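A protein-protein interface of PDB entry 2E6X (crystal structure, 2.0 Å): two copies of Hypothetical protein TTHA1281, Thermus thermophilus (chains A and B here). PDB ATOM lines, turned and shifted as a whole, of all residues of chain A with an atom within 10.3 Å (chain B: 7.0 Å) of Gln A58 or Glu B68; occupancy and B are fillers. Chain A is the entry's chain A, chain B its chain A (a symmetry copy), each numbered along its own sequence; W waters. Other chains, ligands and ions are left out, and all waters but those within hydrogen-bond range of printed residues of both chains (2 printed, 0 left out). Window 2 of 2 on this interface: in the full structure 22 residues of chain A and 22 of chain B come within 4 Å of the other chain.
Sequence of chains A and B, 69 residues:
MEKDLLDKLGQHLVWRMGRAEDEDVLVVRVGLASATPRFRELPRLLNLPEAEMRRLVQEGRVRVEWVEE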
ATOM      1  N   ASP A  24     -11.766 -18.432 -36.223  1.00  0.00           N
ATOM      2  CA  ASP A  24     -10.489 -17.763 -36.241  1.00  0.00           C
ATOM      3  C   ASP A  24     -10.149 -17.278 -34.822  1.00  0.00           C
ATOM      4  O   ASP A  24     -10.118 -16.091 -34.558  1.00  0.00           O
ATOM      5  CB  ASP A  24     -10.584 -16.605 -37.229  1.00  0.00           C
ATOM      6  CG  ASP A  24      -9.245 -15.986 -37.513  1.00  0.00           C
ATOM      7  OD1 ASP A  24      -8.295 -16.751 -37.697  1.00  0.00           O
ATOM      8  OD2 ASP A  24      -9.146 -14.754 -37.535  1.00  0.00           O
ATOM      9  N   LEU A  26      -7.486 -18.009 -31.284  1.00  0.00           N
ATOM     10  CA  LEU A  26      -6.356 -18.693 -30.660  1.00  0.00           C
ATOM     11  C   LEU A  26      -6.857 -19.231 -29.318  1.00  0.00           C
ATOM     12  O   LEU A  26      -7.404 -18.479 -28.514  1.00  0.00           O
ATOM     13  CB  LEU A  26      -5.171 -17.748 -30.397  1.00  0.00           C
ATOM     14  CG  LEU A  26      -4.093 -18.455 -29.534  1.00  0.00           C
ATOM     15  CD1 LEU A  26      -3.320 -19.471 -30.437  1.00  0.00           C
ATOM     16  CD2 LEU A  26      -3.123 -17.435 -28.926  1.00  0.00           C
ATOM     17  N   GLU A  50       3.765 -18.722 -35.861  1.00  0.00           N
ATOM     18  CA  GLU A  50       3.916 -17.811 -34.746  1.00  0.00           C
ATOM     19  C   GLU A  50       3.344 -16.401 -35.086  1.00  0.00           C
ATOM     20  O   GLU A  50       2.789 -15.702 -34.218  1.00  0.00           O
ATOM     21  CB  GLU A  50       5.405 -17.729 -34.361  1.00  0.00           C
ATOM     22  CG  GLU A  50       5.704 -16.676 -33.333  1.00  0.00           C
ATOM     23  CD  GLU A  50       5.950 -15.290 -33.921  1.00  0.00           C
ATOM     24  OE1 GLU A  50       6.187 -15.165 -35.135  1.00  0.00           O
ATOM     25  OE2 GLU A  50       5.938 -14.320 -33.145  1.00  0.00           O
ATOM     26  N   ALA A  51       3.469 -15.994 -36.347  1.00  0.00           N
ATOM     27  CA  ALA A  51       2.949 -14.685 -36.793  1.00  0.00           C
ATOM     28  C   ALA A  51       1.432 -14.608 -36.698  1.00  0.00           C
ATOM     29  O   ALA A  51       0.848 -13.538 -36.392  1.00  0.00           O
ATOM     30  CB  ALA A  51       3.384 -14.417 -38.234  1.00  0.00           C
ATOM     31  N   GLU A  52       0.793 -15.743 -36.979  1.00  0.00           N
ATOM     32  CA  GLU A  52      -0.643 -15.810 -36.895  1.00  0.00           C
ATOM     33  C   GLU A  52      -1.016 -15.677 -35.417  1.00  0.00           C
ATOM     34  O   GLU A  52      -1.996 -15.042 -35.094  1.00  0.00           O
ATOM     35  CB  GLU A  52      -1.203 -17.138 -37.433  1.00  0.00           C
ATOM     36  CG  GLU A  52      -2.709 -16.981 -37.746  1.00  0.00           C
ATOM     37  CD  GLU A  52      -3.441 -18.243 -38.210  1.00  0.00           C
ATOM     38  OE1 GLU A  52      -2.860 -19.105 -38.914  1.00  0.00           O
ATOM     39  OE2 GLU A  52      -4.641 -18.356 -37.869  1.00  0.00           O
ATOM     40  N   MET A  53      -0.261 -16.334 -34.542  1.00  0.00           N
ATOM     41  CA  MET A  53      -0.522 -16.251 -33.106  1.00  0.00           C
ATOM     42  C   MET A  53      -0.390 -14.817 -32.635  1.00  0.00           C
ATOM     43  O   MET A  53      -1.191 -14.361 -31.842  1.00  0.00           O
ATOM     44  CB  MET A  53       0.441 -17.122 -32.289  1.00  0.00           C
ATOM     45  CG  MET A  53       0.257 -18.621 -32.455  1.00  0.00           C
ATOM     46  SD  MET A  53       1.349 -19.585 -31.133  1.00  0.00           S
ATOM     47  CE  MET A  53       1.773 -18.046 -30.033  1.00  0.00           C
ATOM     48  N   ARG A  54       0.600 -14.092 -33.146  1.00  0.00           N
ATOM     49  CA  ARG A  54       0.768 -12.723 -32.706  1.00  0.00           C
ATOM     50  C   ARG A  54      -0.463 -11.908 -33.136  1.00  0.00           C
ATOM     51  O   ARG A  54      -1.040 -11.171 -32.346  1.00  0.00           O
ATOM     52  CB  ARG A  54       2.077 -12.127 -33.288  1.00  0.00           C
ATOM     53  CG  ARG A  54       2.180 -10.630 -33.150  1.00  0.00           C
ATOM     54  CD  ARG A  54       3.466 -10.124 -33.846  1.00  0.00           C
ATOM     55  NE  ARG A  54       3.544  -8.668 -33.861  1.00  0.00           N
ATOM     56  CZ  ARG A  54       3.063  -7.901 -34.839  1.00  0.00           C
ATOM     57  NH1 ARG A  54       2.459  -8.455 -35.909  1.00  0.00           N
ATOM     58  NH2 ARG A  54       3.196  -6.571 -34.758  1.00  0.00           N
ATOM     59  N   ARG A  55      -0.868 -12.078 -34.393  1.00  0.00           N
ATOM     60  CA  ARG A  55      -2.028 -11.372 -34.938  1.00  0.00           C
ATOM     61  C   ARG A  55      -3.299 -11.600 -34.081  1.00  0.00           C
ATOM     62  O   ARG A  55      -4.025 -10.672 -33.720  1.00  0.00           O
ATOM     63  CB  ARG A  55      -2.296 -11.843 -36.377  1.00  0.00           C
ATOM     64  CG  ARG A  55      -3.652 -11.359 -36.933  1.00  0.00           C
ATOM     65  CD  ARG A  55      -3.941 -11.790 -38.385  1.00  0.00           C
ATOM     66  NE  ARG A  55      -4.375 -13.185 -38.540  1.00  0.00           N
ATOM     67  CZ  ARG A  55      -5.589 -13.649 -38.222  1.00  0.00           C
ATOM     68  NH1 ARG A  55      -6.509 -12.831 -37.731  1.00  0.00           N
ATOM     69  NH2 ARG A  55      -5.884 -14.940 -38.389  1.00  0.00           N
ATOM     70  N   LEU A  56      -3.536 -12.854 -33.755  1.00  0.00           N
ATOM     71  CA  LEU A  56      -4.713 -13.226 -32.984  1.00  0.00           C
ATOM     72  C   LEU A  56      -4.674 -12.635 -31.567  1.00  0.00           C
ATOM     73  O   LEU A  56      -5.696 -12.147 -31.064  1.00  0.00           O
ATOM     74  CB  LEU A  56      -4.830 -14.757 -32.994  1.00  0.00           C
ATOM     75  CG  LEU A  56      -5.253 -15.356 -34.362  1.00  0.00           C
ATOM     76  CD1 LEU A  56      -5.135 -16.864 -34.310  1.00  0.00           C
ATOM     77  CD2 LEU A  56      -6.734 -14.953 -34.729  1.00  0.00           C
ATOM     78  N   VAL A  57      -3.514 -12.636 -30.933  1.00  0.00           N
ATOM     79  CA  VAL A  57      -3.439 -12.073 -29.591  1.00  0.00           C
ATOM     80  C   VAL A  57      -3.644 -10.574 -29.719  1.00  0.00           C
ATOM     81  O   VAL A  57      -4.459  -9.996 -29.005  1.00  0.00           O
ATOM     82  CB  VAL A  57      -2.088 -12.372 -28.909  1.00  0.00           C
ATOM     83  CG1 VAL A  57      -2.042 -11.635 -27.495  1.00  0.00           C
ATOM     84  CG2 VAL A  57      -1.965 -13.899 -28.714  1.00  0.00           C
ATOM     85  N   GLN A  58      -2.923  -9.951 -30.638  1.00  0.00           N
ATOM     86  CA  GLN A  58      -3.106  -8.510 -30.815  1.00  0.00           C
ATOM     87  C   GLN A  58      -4.554  -8.117 -31.125  1.00  0.00           C
ATOM     88  O   GLN A  58      -4.998  -7.093 -30.637  1.00  0.00           O
ATOM     89  CB  GLN A  58      -2.153  -7.959 -31.890  1.00  0.00           C
ATOM     90  CG  GLN A  58      -0.691  -8.037 -31.409  1.00  0.00           C
ATOM     91  CD  GLN A  58       0.248  -7.258 -32.283  1.00  0.00           C
ATOM     92  OE1 GLN A  58       0.127  -7.285 -33.485  1.00  0.00           O
ATOM     93  NE2 GLN A  58       1.193  -6.551 -31.671  1.00  0.00           N
ATOM     94  N   GLU A  59      -5.291  -8.894 -31.915  1.00  0.00           N
ATOM     95  CA  GLU A  59      -6.695  -8.501 -32.161  1.00  0.00           C
ATOM     96  C   GLU A  59      -7.642  -8.935 -31.013  1.00  0.00           C
ATOM     97  O   GLU A  59      -8.863  -8.731 -31.070  1.00  0.00           O
ATOM     98  CB  GLU A  59      -7.178  -9.088 -33.479  1.00  0.00           C
ATOM     99  CG  GLU A  59      -6.240  -8.775 -34.629  1.00  0.00           C
ATOM    100  CD  GLU A  59      -6.631  -9.445 -35.922  1.00  0.00           C
ATOM    101  OE1 GLU A  59      -7.036 -10.632 -35.905  1.00  0.00           O
ATOM    102  OE2 GLU A  59      -6.499  -8.792 -36.972  1.00  0.00           O
ATOM    103  N   GLY A  60      -7.088  -9.515 -29.958  1.00  0.00           N
ATOM    104  CA  GLY A  60      -7.950  -9.951 -28.880  1.00  0.00           C
ATOM    105  C   GLY A  60      -8.768 -11.207 -29.178  1.00  0.00           C
ATOM    106  O   GLY A  60      -9.666 -11.570 -28.386  1.00  0.00           O
ATOM    107  N   ARG A  61      -8.468 -11.897 -30.281  1.00  0.00           N
ATOM    108  CA  ARG A  61      -9.197 -13.152 -30.644  1.00  0.00           C
ATOM    109  C   ARG A  61      -8.536 -14.357 -29.955  1.00  0.00           C
ATOM    110  O   ARG A  61      -7.871 -15.182 -30.615  1.00  0.00           O
ATOM    111  CB  ARG A  61      -9.148 -13.405 -32.161  1.00  0.00           C
ATOM    112  CG  ARG A  61      -9.909 -12.383 -33.003  1.00  0.00           C
ATOM    113  CD  ARG A  61      -9.596 -12.577 -34.474  1.00  0.00           C
ATOM    114  NE  ARG A  61      -9.927 -11.399 -35.262  1.00  0.00           N
ATOM    115  CZ  ARG A  61     -11.171 -10.969 -35.444  1.00  0.00           C
ATOM    116  NH1 ARG A  61     -12.190 -11.631 -34.889  1.00  0.00           N
ATOM    117  NH2 ARG A  61     -11.406  -9.880 -36.175  1.00  0.00           N
ATOM    118  N   VAL A  62      -8.695 -14.443 -28.637  1.00  0.00           N
ATOM    119  CA  VAL A  62      -8.067 -15.494 -27.825  1.00  0.00           C
ATOM    120  C   VAL A  62      -9.047 -15.922 -26.725  1.00  0.00           C
ATOM    121  O   VAL A  62      -9.763 -15.094 -26.161  1.00  0.00           O
ATOM    122  CB  VAL A  62      -6.852 -14.975 -27.041  1.00  0.00           C
ATOM    123  CG1 VAL A  62      -6.077 -16.160 -26.439  1.00  0.00           C
ATOM    124  CG2 VAL A  62      -5.972 -14.163 -27.903  1.00  0.00           C
ATOM    125  N   VAL B  30       2.793 -13.077 -23.674  1.00  0.00           N
ATOM    126  CA  VAL B  30       3.485 -14.002 -24.572  1.00  0.00           C
ATOM    127  C   VAL B  30       4.251 -13.290 -25.698  1.00  0.00           C
ATOM    128  O   VAL B  30       3.804 -12.269 -26.236  1.00  0.00           O
ATOM    129  CB  VAL B  30       2.491 -15.007 -25.197  1.00  0.00           C
ATOM    130  CG1 VAL B  30       1.486 -14.276 -26.117  1.00  0.00           C
ATOM    131  CG2 VAL B  30       3.251 -16.042 -25.999  1.00  0.00           C
ATOM    132  N   GLY B  31       5.409 -13.830 -26.051  1.00  0.00           N
ATOM    133  CA  GLY B  31       6.203 -13.229 -27.106  1.00  0.00           C
ATOM    134  C   GLY B  31       7.310 -14.187 -27.527  1.00  0.00           C
ATOM    135  O   GLY B  31       7.465 -15.252 -26.924  1.00  0.00           O
ATOM    136  N   LEU B  32       8.054 -13.826 -28.563  1.00  0.00           N
ATOM    137  CA  LEU B  32       9.171 -14.666 -28.992  1.00  0.00           C
ATOM    138  C   LEU B  32      10.273 -14.579 -27.962  1.00  0.00           C
ATOM    139  O   LEU B  32      10.348 -13.604 -27.206  1.00  0.00           O
ATOM    140  CB  LEU B  32       9.733 -14.191 -30.328  1.00  0.00           C
ATOM    141  CG  LEU B  32       8.902 -14.491 -31.570  1.00  0.00           C
ATOM    142  CD1 LEU B  32       9.571 -13.859 -32.766  1.00  0.00           C
ATOM    143  CD2 LEU B  32       8.764 -16.008 -31.741  1.00  0.00           C
ATOM    144  N   SER B  34      13.246 -13.775 -28.356  1.00  0.00           N
ATOM    145  CA  SER B  34      14.044 -12.580 -28.585  1.00  0.00           C
ATOM    146  C   SER B  34      13.476 -11.331 -27.893  1.00  0.00           C
ATOM    147  O   SER B  34      14.165 -10.317 -27.773  1.00  0.00           O
ATOM    148  CB  SER B  34      14.192 -12.342 -30.092  1.00  0.00           C
ATOM    149  OG  SER B  34      12.934 -12.352 -30.732  1.00  0.00           O
ATOM    150  N   ALA B  35      12.221 -11.420 -27.437  1.00  0.00           N
ATOM    151  CA  ALA B  35      11.548 -10.314 -26.750  1.00  0.00           C
ATOM    152  C   ALA B  35      11.678 -10.380 -25.219  1.00  0.00           C
ATOM    153  O   ALA B  35      11.146  -9.541 -24.513  1.00  0.00           O
ATOM    154  CB  ALA B  35      10.064 -10.296 -27.121  1.00  0.00           C
ATOM    155  N   THR B  36      12.397 -11.380 -24.727  1.00  0.00           N
ATOM    156  CA  THR B  36      12.577 -11.578 -23.316  1.00  0.00           C
ATOM    157  C   THR B  36      12.964 -10.323 -22.553  1.00  0.00           C
ATOM    158  O   THR B  36      12.375 -10.002 -21.537  1.00  0.00           O
ATOM    159  CB  THR B  36      13.643 -12.651 -23.074  1.00  0.00           C
ATOM    160  OG1 THR B  36      13.214 -13.872 -23.679  1.00  0.00           O
ATOM    161  CG2 THR B  36      13.877 -12.844 -21.569  1.00  0.00           C
ATOM    162  N   ARG B  38      12.266  -7.348 -22.963  1.00  0.00           N
ATOM    163  CA  ARG B  38      11.112  -6.428 -22.768  1.00  0.00           C
ATOM    164  C   ARG B  38      10.123  -6.777 -21.665  1.00  0.00           C
ATOM    165  O   ARG B  38       9.420  -5.899 -21.140  1.00  0.00           O
ATOM    166  CB  ARG B  38      10.306  -6.296 -24.055  1.00  0.00           C
ATOM    167  CG  ARG B  38      11.132  -6.035 -25.296  1.00  0.00           C
ATOM    168  CD  ARG B  38      11.657  -4.649 -25.333  1.00  0.00           C
ATOM    169  NE  ARG B  38      12.546  -4.505 -26.473  1.00  0.00           N
ATOM    170  CZ  ARG B  38      13.340  -3.461 -26.669  1.00  0.00           C
ATOM    171  NH1 ARG B  38      13.347  -2.470 -25.786  1.00  0.00           N
ATOM    172  NH2 ARG B  38      14.111  -3.411 -27.753  1.00  0.00           N
ATOM    173  N   PHE B  39      10.034  -8.053 -21.323  1.00  0.00           N
ATOM    174  CA  PHE B  39       9.084  -8.460 -20.307  1.00  0.00           C
ATOM    175  C   PHE B  39       9.298  -7.752 -18.972  1.00  0.00           C
ATOM    176  O   PHE B  39       8.342  -7.252 -18.377  1.00  0.00           O
ATOM    177  CB  PHE B  39       9.110  -9.993 -20.099  1.00  0.00           C
ATOM    178  CG  PHE B  39       8.391 -10.784 -21.182  1.00  0.00           C
ATOM    179  CD1 PHE B  39       8.965 -10.960 -22.441  1.00  0.00           C
ATOM    180  CD2 PHE B  39       7.159 -11.402 -20.915  1.00  0.00           C
ATOM    181  CE1 PHE B  39       8.337 -11.747 -23.420  1.00  0.00           C
ATOM    182  CE2 PHE B  39       6.525 -12.182 -21.881  1.00  0.00           C
ATOM    183  CZ  PHE B  39       7.118 -12.353 -23.143  1.00  0.00           C
ATOM    184  N   ARG B  63      -6.554 -11.530 -19.666  1.00  0.00           N
ATOM    185  CA  ARG B  63      -6.134 -10.700 -20.752  1.00  0.00           C
ATOM    186  C   ARG B  63      -4.816 -11.279 -21.250  1.00  0.00           C
ATOM    187  O   ARG B  63      -3.858 -11.418 -20.490  1.00  0.00           O
ATOM    188  CB  ARG B  63      -5.923  -9.270 -20.305  1.00  0.00           C
ATOM    189  CG  ARG B  63      -5.345  -8.381 -21.441  1.00  0.00           C
ATOM    190  CD  ARG B  63      -5.364  -6.899 -21.065  1.00  0.00           C
ATOM    191  NE  ARG B  63      -4.636  -6.099 -22.062  1.00  0.00           N
ATOM    192  CZ  ARG B  63      -5.182  -5.682 -23.199  1.00  0.00           C
ATOM    193  NH1 ARG B  63      -6.463  -5.980 -23.499  1.00  0.00           N
ATOM    194  NH2 ARG B  63      -4.470  -4.933 -24.026  1.00  0.00           N
ATOM    195  N   VAL B  64      -4.787 -11.647 -22.506  1.00  0.00           N
ATOM    196  CA  VAL B  64      -3.544 -12.187 -23.082  1.00  0.00           C
ATOM    197  C   VAL B  64      -2.863 -11.029 -23.813  1.00  0.00           C
ATOM    198  O   VAL B  64      -3.494 -10.305 -24.594  1.00  0.00           O
ATOM    199  CB  VAL B  64      -3.819 -13.336 -24.032  1.00  0.00           C
ATOM    200  CG1 VAL B  64      -2.441 -13.872 -24.667  1.00  0.00           C
ATOM    201  CG2 VAL B  64      -4.515 -14.440 -23.235  1.00  0.00           C
ATOM    202  N   GLU B  65      -1.574 -10.873 -23.567  1.00  0.00           N
ATOM    203  CA  GLU B  65      -0.819  -9.737 -24.110  1.00  0.00           C
ATOM    204  C   GLU B  65       0.380 -10.134 -24.941  1.00  0.00           C
ATOM    205  O   GLU B  65       1.182 -10.964 -24.502  1.00  0.00           O
ATOM    206  CB  GLU B  65      -0.358  -8.845 -22.915  1.00  0.00           C
ATOM    207  CG  GLU B  65      -1.532  -8.244 -22.141  1.00  0.00           C
ATOM    208  CD  GLU B  65      -1.114  -7.472 -20.892  1.00  0.00           C
ATOM    209  OE1 GLU B  65       0.116  -7.315 -20.624  1.00  0.00           O
ATOM    210  OE2 GLU B  65      -2.029  -7.014 -20.168  1.00  0.00           O
ATOM    211  N   TRP B  66       0.551  -9.501 -26.103  1.00  0.00           N
ATOM    212  CA  TRP B  66       1.684  -9.863 -26.940  1.00  0.00           C
ATOM    213  C   TRP B  66       2.794  -8.859 -26.716  1.00  0.00           C
ATOM    214  O   TRP B  66       2.574  -7.651 -26.762  1.00  0.00           O
ATOM    215  CB  TRP B  66       1.302  -9.895 -28.424  1.00  0.00           C
ATOM    216  CG  TRP B  66       2.453 -10.313 -29.274  1.00  0.00           C
ATOM    217  CD1 TRP B  66       3.380  -9.503 -29.889  1.00  0.00           C
ATOM    218  CD2 TRP B  66       2.838 -11.651 -29.551  1.00  0.00           C
ATOM    219  NE1 TRP B  66       4.319 -10.275 -30.544  1.00  0.00           N
ATOM    220  CE2 TRP B  66       4.013 -11.597 -30.345  1.00  0.00           C
ATOM    221  CE3 TRP B  66       2.302 -12.902 -29.216  1.00  0.00           C
ATOM    222  CZ2 TRP B  66       4.670 -12.747 -30.786  1.00  0.00           C
ATOM    223  CZ3 TRP B  66       2.958 -14.043 -29.655  1.00  0.00           C
ATOM    224  CH2 TRP B  66       4.125 -13.950 -30.436  1.00  0.00           C
ATOM    225  N   VAL B  67       3.981  -9.369 -26.437  1.00  0.00           N
ATOM    226  CA  VAL B  67       5.136  -8.531 -26.186  1.00  0.00           C
ATOM    227  C   VAL B  67       6.021  -8.507 -27.404  1.00  0.00           C
ATOM    228  O   VAL B  67       6.607  -9.520 -27.741  1.00  0.00           O
ATOM    229  CB  VAL B  67       5.971  -9.102 -25.042  1.00  0.00           C
ATOM    230  CG1 VAL B  67       7.140  -8.195 -24.790  1.00  0.00           C
ATOM    231  CG2 VAL B  67       5.100  -9.284 -23.776  1.00  0.00           C
ATOM    232  N   GLU B  68       6.115  -7.349 -28.058  1.00  0.00           N
ATOM    233  CA  GLU B  68       6.905  -7.178 -29.261  1.00  0.00           C
ATOM    234  C   GLU B  68       8.395  -7.210 -28.906  1.00  0.00           C
ATOM    235  O   GLU B  68       8.807  -6.675 -27.857  1.00  0.00           O
ATOM    236  CB  GLU B  68       6.579  -5.821 -29.909  1.00  0.00           C
ATOM    237  CG  GLU B  68       5.114  -5.585 -30.215  1.00  0.00           C
ATOM    238  CD  GLU B  68       4.705  -6.046 -31.595  1.00  0.00           C
ATOM    239  OE1 GLU B  68       4.077  -5.219 -32.314  1.00  0.00           O
ATOM    240  OE2 GLU B  68       4.991  -7.216 -31.958  1.00  0.00           O
ATOM    241  N   GLU B  69       9.202  -7.856 -29.747  1.00  0.00           N
ATOM    242  CA  GLU B  69      10.632  -7.897 -29.457  1.00  0.00           C
ATOM    243  C   GLU B  69      11.315  -6.599 -29.878  1.00  0.00           C
ATOM    244  O   GLU B  69      12.381  -6.307 -29.304  1.00  0.00           O
ATOM    245  CB  GLU B  69      11.305  -9.110 -30.105  1.00  0.00           C
ATOM    246  CG  GLU B  69      10.520  -9.790 -31.206  1.00  0.00           C
ATOM    247  CD  GLU B  69      10.528  -8.989 -32.483  1.00  0.00           C
ATOM    248  OE1 GLU B  69      10.069  -9.510 -33.523  1.00  0.00           O
ATOM    249  OE2 GLU B  69      11.004  -7.830 -32.445  1.00  0.00           O
ATOM    250  OXT GLU B  69      10.758  -5.866 -30.750  1.00  0.00           O
HETATM  251  O   HOH W   1       1.519  -6.189 -28.805  1.00  0.00           O
HETATM  252  O   HOH W   2      -5.355 -10.687 -26.529  1.00  0.00           O
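Printed residues of chain B that touch a printed residue of chain A: Leu B32, Val B64, Glu B65, Trp B66 and Glu B68. Hydrophobic or aromatic side chains of chain B within 4 Å of the printed part of chain A: Leu B32, Val B64 and Trp B66. Along chain B the printed residues that touch a printed residue of chain A span positions 32 to 68. Of the 15 printed residues of chain A, 5 touch a printed residue of chain B. Printed residues of chain A that touch a printed residue of chain B: Glu A50, Arg A54, Val A57, Gln A58 and Val A62. Hydrophobic or aromatic side chains of chain A that line the printed part of chain B: Val A57 and Val A62. Along chain A the printed residues that touch a printed residue of chain B span positions 50 to 62. Among the printed residues, 9 pairs touch across the chains. Among the printed residues, Asp or Glu carboxylates within 4 Å of a Lys or Arg side-chain nitrogen of the other chain: Arg A54 with Glu B68 (2.8 Å).
NE2 of Gln A58 lies within hydrogen-bond range of OE1 of Glu B68 (3.2 Å). The guanidinium group (NE) of Arg A54 lies within salt-bridge range of the side-chain carboxylate (OE2) of Glu B68 (2.8 Å).
Water W2 bridges the backbone carbonyl oxygen of Val B64 (2.7 Å) and the backbone carbonyl oxygen of Val A57 (2.7 Å). Water W1 bridges O of Trp B66 (2.7 Å) and NE2 of Gln A58 (2.9 Å).
N of Val B30 lies within hydrogen-bond range of O of Glu B65 (2.8 Å). NE1 of Trp B66 sits at hydrogen-bond distance from OE2 of Glu B68, at 3.4 Å. The guanidinium group (NE) of Arg B63 is in salt-bridge range of the side-chain carboxylate (OE2) of Glu B65 (3.3 Å). NH2 of Arg A54 lies close to OE1 of Gln A58 (3.4 Å).
Glu A50 touches Leu B32 (OE2 to CG, 3.4 Å). CZ2 of Trp B66 touches OE2 of Glu A50, 3.1 Å away. Arg A54 touches Trp B66 (CG to NE1, 3.4 Å). Val A57 touches Val B64 (CG1 to O, 3.5 Å). CG1 of Val A57 touches C of Glu B65, 3.8 Å away. Trp B66 touches Val A57 (N to CG1, 3.6 Å). Val A62 touches Val B64 (CG1 to CG2, 3.96 Å).
No position is printed for both chains. Of the 9 pairs that touch across the chains among the printed residues, none has its exchanged pair printed and touching as well.
Of chain B, only Glu B68 comes within 4 Å of Gln A58. Glu B68 touches just these residues of chain A: Arg A54 and Gln A58. No residue of chain A comes within 4 Å of Val B67. No residue of chain A comes within 4 Å of Glu B69. Printed residues of chain B within 4 Å of Val A62: Val B64 (3.96 Å). Of the printed residues of chain A, Leu B32 touches Glu A50 (3.4 Å). Printed residues of chain B within 4 Å of Val A57: Val B64 (3.5 Å), Glu B65 (3.8 Å) and Trp B66 (3.6 Å). Glu A59 touches none of the printed residues of chain B. Ser B34 touches none of the printed residues of chain A. The nearest residue of chain B that does not touch Gln A58 is Trp B66 (4.04 Å). The nearest residue of chain A that does not touch Glu B68 is Glu A50 (7.3 Å).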
